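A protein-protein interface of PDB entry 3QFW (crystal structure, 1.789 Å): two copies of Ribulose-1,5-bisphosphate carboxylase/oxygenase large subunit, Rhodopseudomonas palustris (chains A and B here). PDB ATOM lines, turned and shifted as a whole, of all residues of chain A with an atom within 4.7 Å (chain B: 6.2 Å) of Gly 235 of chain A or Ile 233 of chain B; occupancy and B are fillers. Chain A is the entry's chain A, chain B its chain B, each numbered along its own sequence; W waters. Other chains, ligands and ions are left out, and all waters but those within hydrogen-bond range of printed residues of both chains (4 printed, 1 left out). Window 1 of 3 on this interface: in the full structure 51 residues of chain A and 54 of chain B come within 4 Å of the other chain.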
ATOM      1  N   GLY A  81      30.372  17.135  -5.374  1.00  0.00           N
ATOM      2  CA  GLY A  81      29.686  15.975  -4.807  1.00  0.00           C
ATOM      3  C   GLY A  81      29.183  16.189  -3.384  1.00  0.00           C
ATOM      4  O   GLY A  81      28.030  15.894  -3.057  1.00  0.00           O
ATOM      5  N   ASN A  85      25.557  16.378  -1.890  1.00  0.00           N
ATOM      6  CA  ASN A  85      25.302  15.594  -0.675  1.00  0.00           C
ATOM      7  C   ASN A  85      24.528  16.382   0.380  1.00  0.00           C
ATOM      8  O   ASN A  85      23.441  15.978   0.803  1.00  0.00           O
ATOM      9  CB  ASN A  85      26.625  15.064  -0.094  1.00  0.00           C
ATOM     10  CG  ASN A  85      26.425  13.903   0.909  1.00  0.00           C
ATOM     11  OD1 ASN A  85      25.381  13.245   0.932  1.00  0.00           O
ATOM     12  ND2 ASN A  85      27.438  13.659   1.733  1.00  0.00           N
ATOM     13  N   PRO A 231      27.198  14.945 -16.400  1.00  0.00           N
ATOM     14  CA  PRO A 231      27.737  15.080 -15.036  1.00  0.00           C
ATOM     15  C   PRO A 231      27.121  14.093 -14.049  1.00  0.00           C
ATOM     16  O   PRO A 231      27.810  13.607 -13.137  1.00  0.00           O
ATOM     17  CB  PRO A 231      27.378  16.522 -14.654  1.00  0.00           C
ATOM     18  CG  PRO A 231      27.304  17.259 -16.011  1.00  0.00           C
ATOM     19  CD  PRO A 231      26.690  16.225 -16.934  1.00  0.00           C
ATOM     20  N   MET A 232      25.842  13.788 -14.228  1.00  0.00           N
ATOM     21  CA  MET A 232      25.150  12.940 -13.253  1.00  0.00           C
ATOM     22  C   MET A 232      25.481  11.461 -13.432  1.00  0.00           C
ATOM     23  O   MET A 232      25.252  10.641 -12.536  1.00  0.00           O
ATOM     24  CB  MET A 232      23.647  13.232 -13.264  1.00  0.00           C
ATOM     25  CG  MET A 232      23.333  14.721 -12.988  1.00  0.00           C
ATOM     26  SD  MET A 232      23.863  15.355 -11.368  1.00  0.00           S
ATOM     27  CE  MET A 232      25.575  14.924 -11.284  1.00  0.00           C
ATOM     28  N   ILE A 233      26.058  11.134 -14.581  1.00  0.00           N
ATOM     29  CA  ILE A 233      26.582   9.792 -14.807  1.00  0.00           C
ATOM     30  C   ILE A 233      27.968   9.665 -14.192  1.00  0.00           C
ATOM     31  O   ILE A 233      28.245   8.720 -13.453  1.00  0.00           O
ATOM     32  CB  ILE A 233      26.697   9.467 -16.314  1.00  0.00           C
ATOM     33  CG1 ILE A 233      25.313   9.397 -16.957  1.00  0.00           C
ATOM     34  CG2 ILE A 233      27.430   8.147 -16.521  1.00  0.00           C
ATOM     35  CD1 ILE A 233      24.411   8.342 -16.326  1.00  0.00           C
ATOM     36  N   VAL A 234      28.829  10.637 -14.485  1.00  0.00           N
ATOM     37  CA  VAL A 234      30.253  10.519 -14.169  1.00  0.00           C
ATOM     38  C   VAL A 234      30.602  11.029 -12.776  1.00  0.00           C
ATOM     39  O   VAL A 234      31.711  10.819 -12.290  1.00  0.00           O
ATOM     40  CB  VAL A 234      31.114  11.242 -15.217  1.00  0.00           C
ATOM     41  CG1 VAL A 234      30.746  10.762 -16.623  1.00  0.00           C
ATOM     42  CG2 VAL A 234      30.919  12.743 -15.092  1.00  0.00           C
ATOM     43  N   GLY A 235      29.634  11.655 -12.116  1.00  0.00           N
ATOM     44  CA  GLY A 235      29.853  12.234 -10.804  1.00  0.00           C
ATOM     45  C   GLY A 235      30.220  13.699 -10.973  1.00  0.00           C
ATOM     46  O   GLY A 235      31.185  14.017 -11.668  1.00  0.00           O
ATOM     47  N   VAL A 236      29.460  14.596 -10.353  1.00  0.00           N
ATOM     48  CA  VAL A 236      29.728  16.023 -10.538  1.00  0.00           C
ATOM     49  C   VAL A 236      31.134  16.437 -10.114  1.00  0.00           C
ATOM     50  O   VAL A 236      31.724  17.336 -10.720  1.00  0.00           O
ATOM     51  CB  VAL A 236      28.729  16.919  -9.801  1.00  0.00           C
ATOM     52  CG1 VAL A 236      29.188  18.341  -9.899  1.00  0.00           C
ATOM     53  CG2 VAL A 236      27.374  16.828 -10.422  1.00  0.00           C
ATOM     54  N   SER A 237      31.667  15.814  -9.063  1.00  0.00           N
ATOM     55  CA  SER A 237      33.040  16.111  -8.653  1.00  0.00           C
ATOM     56  C   SER A 237      34.039  15.812  -9.787  1.00  0.00           C
ATOM     57  O   SER A 237      34.951  16.594 -10.046  1.00  0.00           O
ATOM     58  CB  SER A 237      33.416  15.386  -7.349  1.00  0.00           C
ATOM     59  OG  SER A 237      32.749  15.947  -6.224  1.00  0.00           O
ATOM     60  N   ASN A 238      33.855  14.697 -10.486  1.00  0.00           N
ATOM     61  CA  ASN A 238      34.716  14.378 -11.628  1.00  0.00           C
ATOM     62  C   ASN A 238      34.430  15.199 -12.883  1.00  0.00           C
ATOM     63  O   ASN A 238      35.342  15.521 -13.663  1.00  0.00           O
ATOM     64  CB  ASN A 238      34.635  12.884 -11.935  1.00  0.00           C
ATOM     65  CG  ASN A 238      34.877  12.038 -10.706  1.00  0.00           C
ATOM     66  OD1 ASN A 238      35.988  11.998 -10.172  1.00  0.00           O
ATOM     67  ND2 ASN A 238      33.826  11.365 -10.233  1.00  0.00           N
ATOM     68  N   PHE A 239      33.165  15.542 -13.091  1.00  0.00           N
ATOM     69  CA  PHE A 239      32.837  16.460 -14.174  1.00  0.00           C
ATOM     70  C   PHE A 239      33.608  17.765 -13.966  1.00  0.00           C
ATOM     71  O   PHE A 239      34.195  18.315 -14.905  1.00  0.00           O
ATOM     72  CB  PHE A 239      31.331  16.733 -14.240  1.00  0.00           C
ATOM     73  CG  PHE A 239      30.960  17.919 -15.127  1.00  0.00           C
ATOM     74  CD1 PHE A 239      31.070  17.836 -16.511  1.00  0.00           C
ATOM     75  CD2 PHE A 239      30.488  19.096 -14.566  1.00  0.00           C
ATOM     76  CE1 PHE A 239      30.729  18.928 -17.339  1.00  0.00           C
ATOM     77  CE2 PHE A 239      30.143  20.187 -15.362  1.00  0.00           C
ATOM     78  CZ  PHE A 239      30.260  20.106 -16.766  1.00  0.00           C
ATOM     79  N   HIS B 167      27.015   9.900   6.808  1.00  0.00           N
ATOM     80  CA  HIS B 167      27.276   9.965   5.372  1.00  0.00           C
ATOM     81  C   HIS B 167      27.579  11.405   4.976  1.00  0.00           C
ATOM     82  O   HIS B 167      28.106  11.665   3.893  1.00  0.00           O
ATOM     83  CB  HIS B 167      26.070   9.485   4.579  1.00  0.00           C
ATOM     84  CG  HIS B 167      25.027  10.536   4.397  1.00  0.00           C
ATOM     85  ND1 HIS B 167      24.973  11.344   3.279  1.00  0.00           N
ATOM     86  CD2 HIS B 167      24.019  10.939   5.203  1.00  0.00           C
ATOM     87  CE1 HIS B 167      23.968  12.191   3.402  1.00  0.00           C
ATOM     88  NE2 HIS B 167      23.370  11.964   4.559  1.00  0.00           N
ATOM     89  N   SER B 206      35.187  10.523  -0.210  1.00  0.00           N
ATOM     90  CA  SER B 206      34.449  11.587  -0.890  1.00  0.00           C
ATOM     91  C   SER B 206      35.206  12.241  -2.051  1.00  0.00           C
ATOM     92  O   SER B 206      36.427  12.125  -2.157  1.00  0.00           O
ATOM     93  CB  SER B 206      34.149  12.696   0.130  1.00  0.00           C
ATOM     94  OG  SER B 206      32.791  13.062   0.089  1.00  0.00           O
ATOM     95  N   GLY B 207      34.467  12.951  -2.902  1.00  0.00           N
ATOM     96  CA  GLY B 207      35.065  13.838  -3.894  1.00  0.00           C
ATOM     97  C   GLY B 207      35.330  13.199  -5.248  1.00  0.00           C
ATOM     98  O   GLY B 207      34.567  12.349  -5.697  1.00  0.00           O
ATOM     99  N   ALA B 230      29.064   6.591  -1.055  1.00  0.00           N
ATOM    100  CA  ALA B 230      27.765   6.783  -1.696  1.00  0.00           C
ATOM    101  C   ALA B 230      27.941   6.738  -3.209  1.00  0.00           C
ATOM    102  O   ALA B 230      28.357   7.734  -3.812  1.00  0.00           O
ATOM    103  CB  ALA B 230      27.166   8.104  -1.268  1.00  0.00           C
ATOM    104  N   PRO B 231      27.642   5.583  -3.830  1.00  0.00           N
ATOM    105  CA  PRO B 231      27.946   5.399  -5.255  1.00  0.00           C
ATOM    106  C   PRO B 231      27.288   6.454  -6.140  1.00  0.00           C
ATOM    107  O   PRO B 231      27.886   6.869  -7.139  1.00  0.00           O
ATOM    108  CB  PRO B 231      27.393   3.994  -5.564  1.00  0.00           C
ATOM    109  CG  PRO B 231      27.405   3.278  -4.202  1.00  0.00           C
ATOM    110  CD  PRO B 231      27.077   4.361  -3.211  1.00  0.00           C
ATOM    111  N   MET B 232      26.093   6.907  -5.773  1.00  0.00           N
ATOM    112  CA  MET B 232      25.361   7.820  -6.641  1.00  0.00           C
ATOM    113  C   MET B 232      25.878   9.247  -6.513  1.00  0.00           C
ATOM    114  O   MET B 232      25.602  10.095  -7.359  1.00  0.00           O
ATOM    115  CB  MET B 232      23.847   7.707  -6.423  1.00  0.00           C
ATOM    116  CG  MET B 232      23.300   6.266  -6.650  1.00  0.00           C
ATOM    117  SD  MET B 232      23.553   5.594  -8.319  1.00  0.00           S
ATOM    118  CE  MET B 232      25.307   5.698  -8.495  1.00  0.00           C
ATOM    119  N   ILE B 233      26.650   9.498  -5.462  1.00  0.00           N
ATOM    120  CA  ILE B 233      27.364  10.760  -5.349  1.00  0.00           C
ATOM    121  C   ILE B 233      28.626  10.752  -6.197  1.00  0.00           C
ATOM    122  O   ILE B 233      28.832  11.641  -7.022  1.00  0.00           O
ATOM    123  CB  ILE B 233      27.752  11.075  -3.906  1.00  0.00           C
ATOM    124  CG1 ILE B 233      26.501  11.344  -3.083  1.00  0.00           C
ATOM    125  CG2 ILE B 233      28.680  12.308  -3.860  1.00  0.00           C
ATOM    126  CD1 ILE B 233      26.780  11.560  -1.633  1.00  0.00           C
ATOM    127  N   VAL B 234      29.448   9.721  -6.015  1.00  0.00           N
ATOM    128  CA  VAL B 234      30.804   9.720  -6.544  1.00  0.00           C
ATOM    129  C   VAL B 234      30.888   9.145  -7.950  1.00  0.00           C
ATOM    130  O   VAL B 234      31.942   9.186  -8.584  1.00  0.00           O
ATOM    131  CB  VAL B 234      31.737   8.941  -5.629  1.00  0.00           C
ATOM    132  CG1 VAL B 234      31.594   9.452  -4.192  1.00  0.00           C
ATOM    133  CG2 VAL B 234      31.398   7.451  -5.690  1.00  0.00           C
ATOM    134  N   GLY B 235      29.769   8.634  -8.449  1.00  0.00           N
ATOM    135  CA  GLY B 235      29.741   8.024  -9.764  1.00  0.00           C
ATOM    136  C   GLY B 235      29.959   6.529  -9.613  1.00  0.00           C
ATOM    137  O   GLY B 235      30.947   6.092  -9.010  1.00  0.00           O
ATOM    138  N   ASN B 238      33.357   5.168 -10.670  1.00  0.00           N
ATOM    139  CA  ASN B 238      34.410   5.377  -9.672  1.00  0.00           C
ATOM    140  C   ASN B 238      34.246   4.546  -8.398  1.00  0.00           C
ATOM    141  O   ASN B 238      35.234   4.093  -7.791  1.00  0.00           O
ATOM    142  CB  ASN B 238      34.507   6.860  -9.350  1.00  0.00           C
ATOM    143  CG  ASN B 238      34.644   7.687 -10.592  1.00  0.00           C
ATOM    144  OD1 ASN B 238      35.639   7.584 -11.312  1.00  0.00           O
ATOM    145  ND2 ASN B 238      33.628   8.495 -10.880  1.00  0.00           N
ATOM    146  N   HIS B 254      26.273   3.570   0.748  1.00  0.00           N
ATOM    147  CA  HIS B 254      25.241   4.459   1.278  1.00  0.00           C
ATOM    148  C   HIS B 254      24.369   4.980   0.129  1.00  0.00           C
ATOM    149  O   HIS B 254      24.863   5.210  -0.978  1.00  0.00           O
ATOM    150  CB  HIS B 254      25.882   5.652   1.994  1.00  0.00           C
ATOM    151  CG  HIS B 254      24.899   6.514   2.725  1.00  0.00           C
ATOM    152  ND1 HIS B 254      24.261   7.584   2.135  1.00  0.00           N
ATOM    153  CD2 HIS B 254      24.431   6.452   3.998  1.00  0.00           C
ATOM    154  CE1 HIS B 254      23.446   8.147   3.009  1.00  0.00           C
ATOM    155  NE2 HIS B 254      23.535   7.482   4.152  1.00  0.00           N
ATOM    156  N   ALA B 256      22.860   7.872  -0.526  1.00  0.00           N
ATOM    157  CA  ALA B 256      22.733   9.302  -0.812  1.00  0.00           C
ATOM    158  C   ALA B 256      22.575   9.552  -2.320  1.00  0.00           C
ATOM    159  O   ALA B 256      23.356   9.042  -3.111  1.00  0.00           O
ATOM    160  CB  ALA B 256      23.937  10.057  -0.274  1.00  0.00           C
ATOM    161  N   MET B 257      21.553  10.329  -2.685  1.00  0.00           N
ATOM    162  CA  MET B 257      21.228  10.689  -4.085  1.00  0.00           C
ATOM    163  C   MET B 257      20.674   9.551  -4.946  1.00  0.00           C
ATOM    164  O   MET B 257      20.588   9.679  -6.169  1.00  0.00           O
ATOM    165  CB  MET B 257      22.392  11.408  -4.789  1.00  0.00           C
ATOM    166  CG  MET B 257      22.486  12.920  -4.493  1.00  0.00           C
ATOM    167  SD  MET B 257      21.169  13.947  -5.230  1.00  0.00           S
ATOM    168  CE  MET B 257      21.532  13.692  -6.956  1.00  0.00           C
HETATM  169  O   HOH W   1      34.484  10.190  -7.562  1.00  0.00           O
HETATM  170  O   HOH W   2      33.999   9.667 -13.637  1.00  0.00           O
HETATM  171  O   HOH W   3      30.857  13.422  -7.664  1.00  0.00           O
HETATM  172  O   HOH W   4      27.451  13.267  -8.684  1.00  0.00           O
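O of His 167 of chain B is in hydrogen-bond range of ND2 of Asn 85 of chain A (3.0 Å).
The backbone carbonyl oxygen (O) of Val 234 of chain A is in hydrogen-bond range of the side-chain amide nitrogen (ND2) of Asn 238 of chain B.
The backbone carbonyl oxygen (O) of Val 234 of chain B sits at hydrogen-bond distance from the side-chain amide nitrogen (ND2) of Asn 238 of chain A (3.3 Å).
The side-chain amide nitrogen (ND2) of Asn 238 of chain A sits close to the side-chain amide nitrogen (ND2) of Asn 238 of chain B (2.9 Å).
N of Gly 81 of chain A sits at hydrogen-bond distance from OG of Ser 237 of chain A, 2.8 Å away.
The backbone carbonyl oxygen (O) of Val 234 of chain A is in hydrogen-bond range of the side-chain amide nitrogen (ND2) of Asn 238 of chain A.
O of Val 234 of chain B is in hydrogen-bond range of ND2 of Asn 238 of chain B (2.9 Å).
A ring nitrogen (ND1) of His 254 of chain B sits at hydrogen-bond distance from the backbone NH (N) of Ala 256 of chain B (3.0 Å).
Among the printed residues, pairs that only touch across the chains: Gly 81 of chain A with Ile 233 of chain B (3.7 Å), Asn 85 of chain A with Ile 233 of chain B (3.4 Å), Asn 85 of chain A with Ala 256 of chain B (3.7 Å), Gly 235 of chain A with Ile 233 of chain B (3.96 Å) and Ser 237 of chain A with Gly 207 of chain B (3.6 Å).
Of chain B, only Ile 233 (3.96 Å) comes within 4 Å of Gly 235 of chain A.
Printed residues of chain A within 4 Å of Asn 238 of chain B: Val 234 and Asn 238.
Of the printed residues of chain B, Asn 85 of chain A touches His 167, Ile 233 and Ala 256.
Gly 235 of chain B touches none of the printed residues of chain A.
Pro 231 of chain B touches none of the printed residues of chain A.
Hydrophobic or aromatic side chains of chain B within 4 Å of the printed part of chain A: His 167, Ile 233 and Ala 256.
Of the 11 printed residues of chain A, 6 touch a printed residue of chain B.
Printed residues of chain A that touch a printed residue of chain B: Gly 81, Asn 85, Val 234, Gly 235, Ser 237 and Asn 238.
Among the printed residues, no Asp or Glu carboxylate lies within 4 Å of a Lys or Arg side-chain nitrogen of the other chain.
Val 234 of chain A touches Asn 238 of chain B, and with the chains exchanged Asn 238 of chain A touches Val 234 of chain B.
Gly 235 of chain A touches Ile 233 of chain B, but with the chains exchanged Ile 233 of chain A does not touch Gly 235 of chain B (4.04 Å).
Asn 238 of chain B touches its own counterpart, Asn 238 of chain A.
Positions printed for both chains: 231, 232, 233, 234, 235 and 238.
Water W4 bridges O of Ile 233 of chain B (2.7 Å) and N of Val 236 of chain A (2.9 Å).
Water W3 lies within hydrogen-bond range of the backbone carbonyl oxygen of Ile 233 of chain B (2.8 Å), the backbone NH of Ser 237 of chain A (2.9 Å) and the backbone NH of Val 236 of chain A (3.2 Å).
Water W1 lies within hydrogen-bond range of the backbone carbonyl oxygen of Gly 207 of chain B, the backbone carbonyl oxygen of Val 234 of chain B and the side-chain amide nitrogen of Asn 238 of chain A.
Water W2 bridges O of Val 234 of chain A and ND2 of Asn 238 of chain B.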
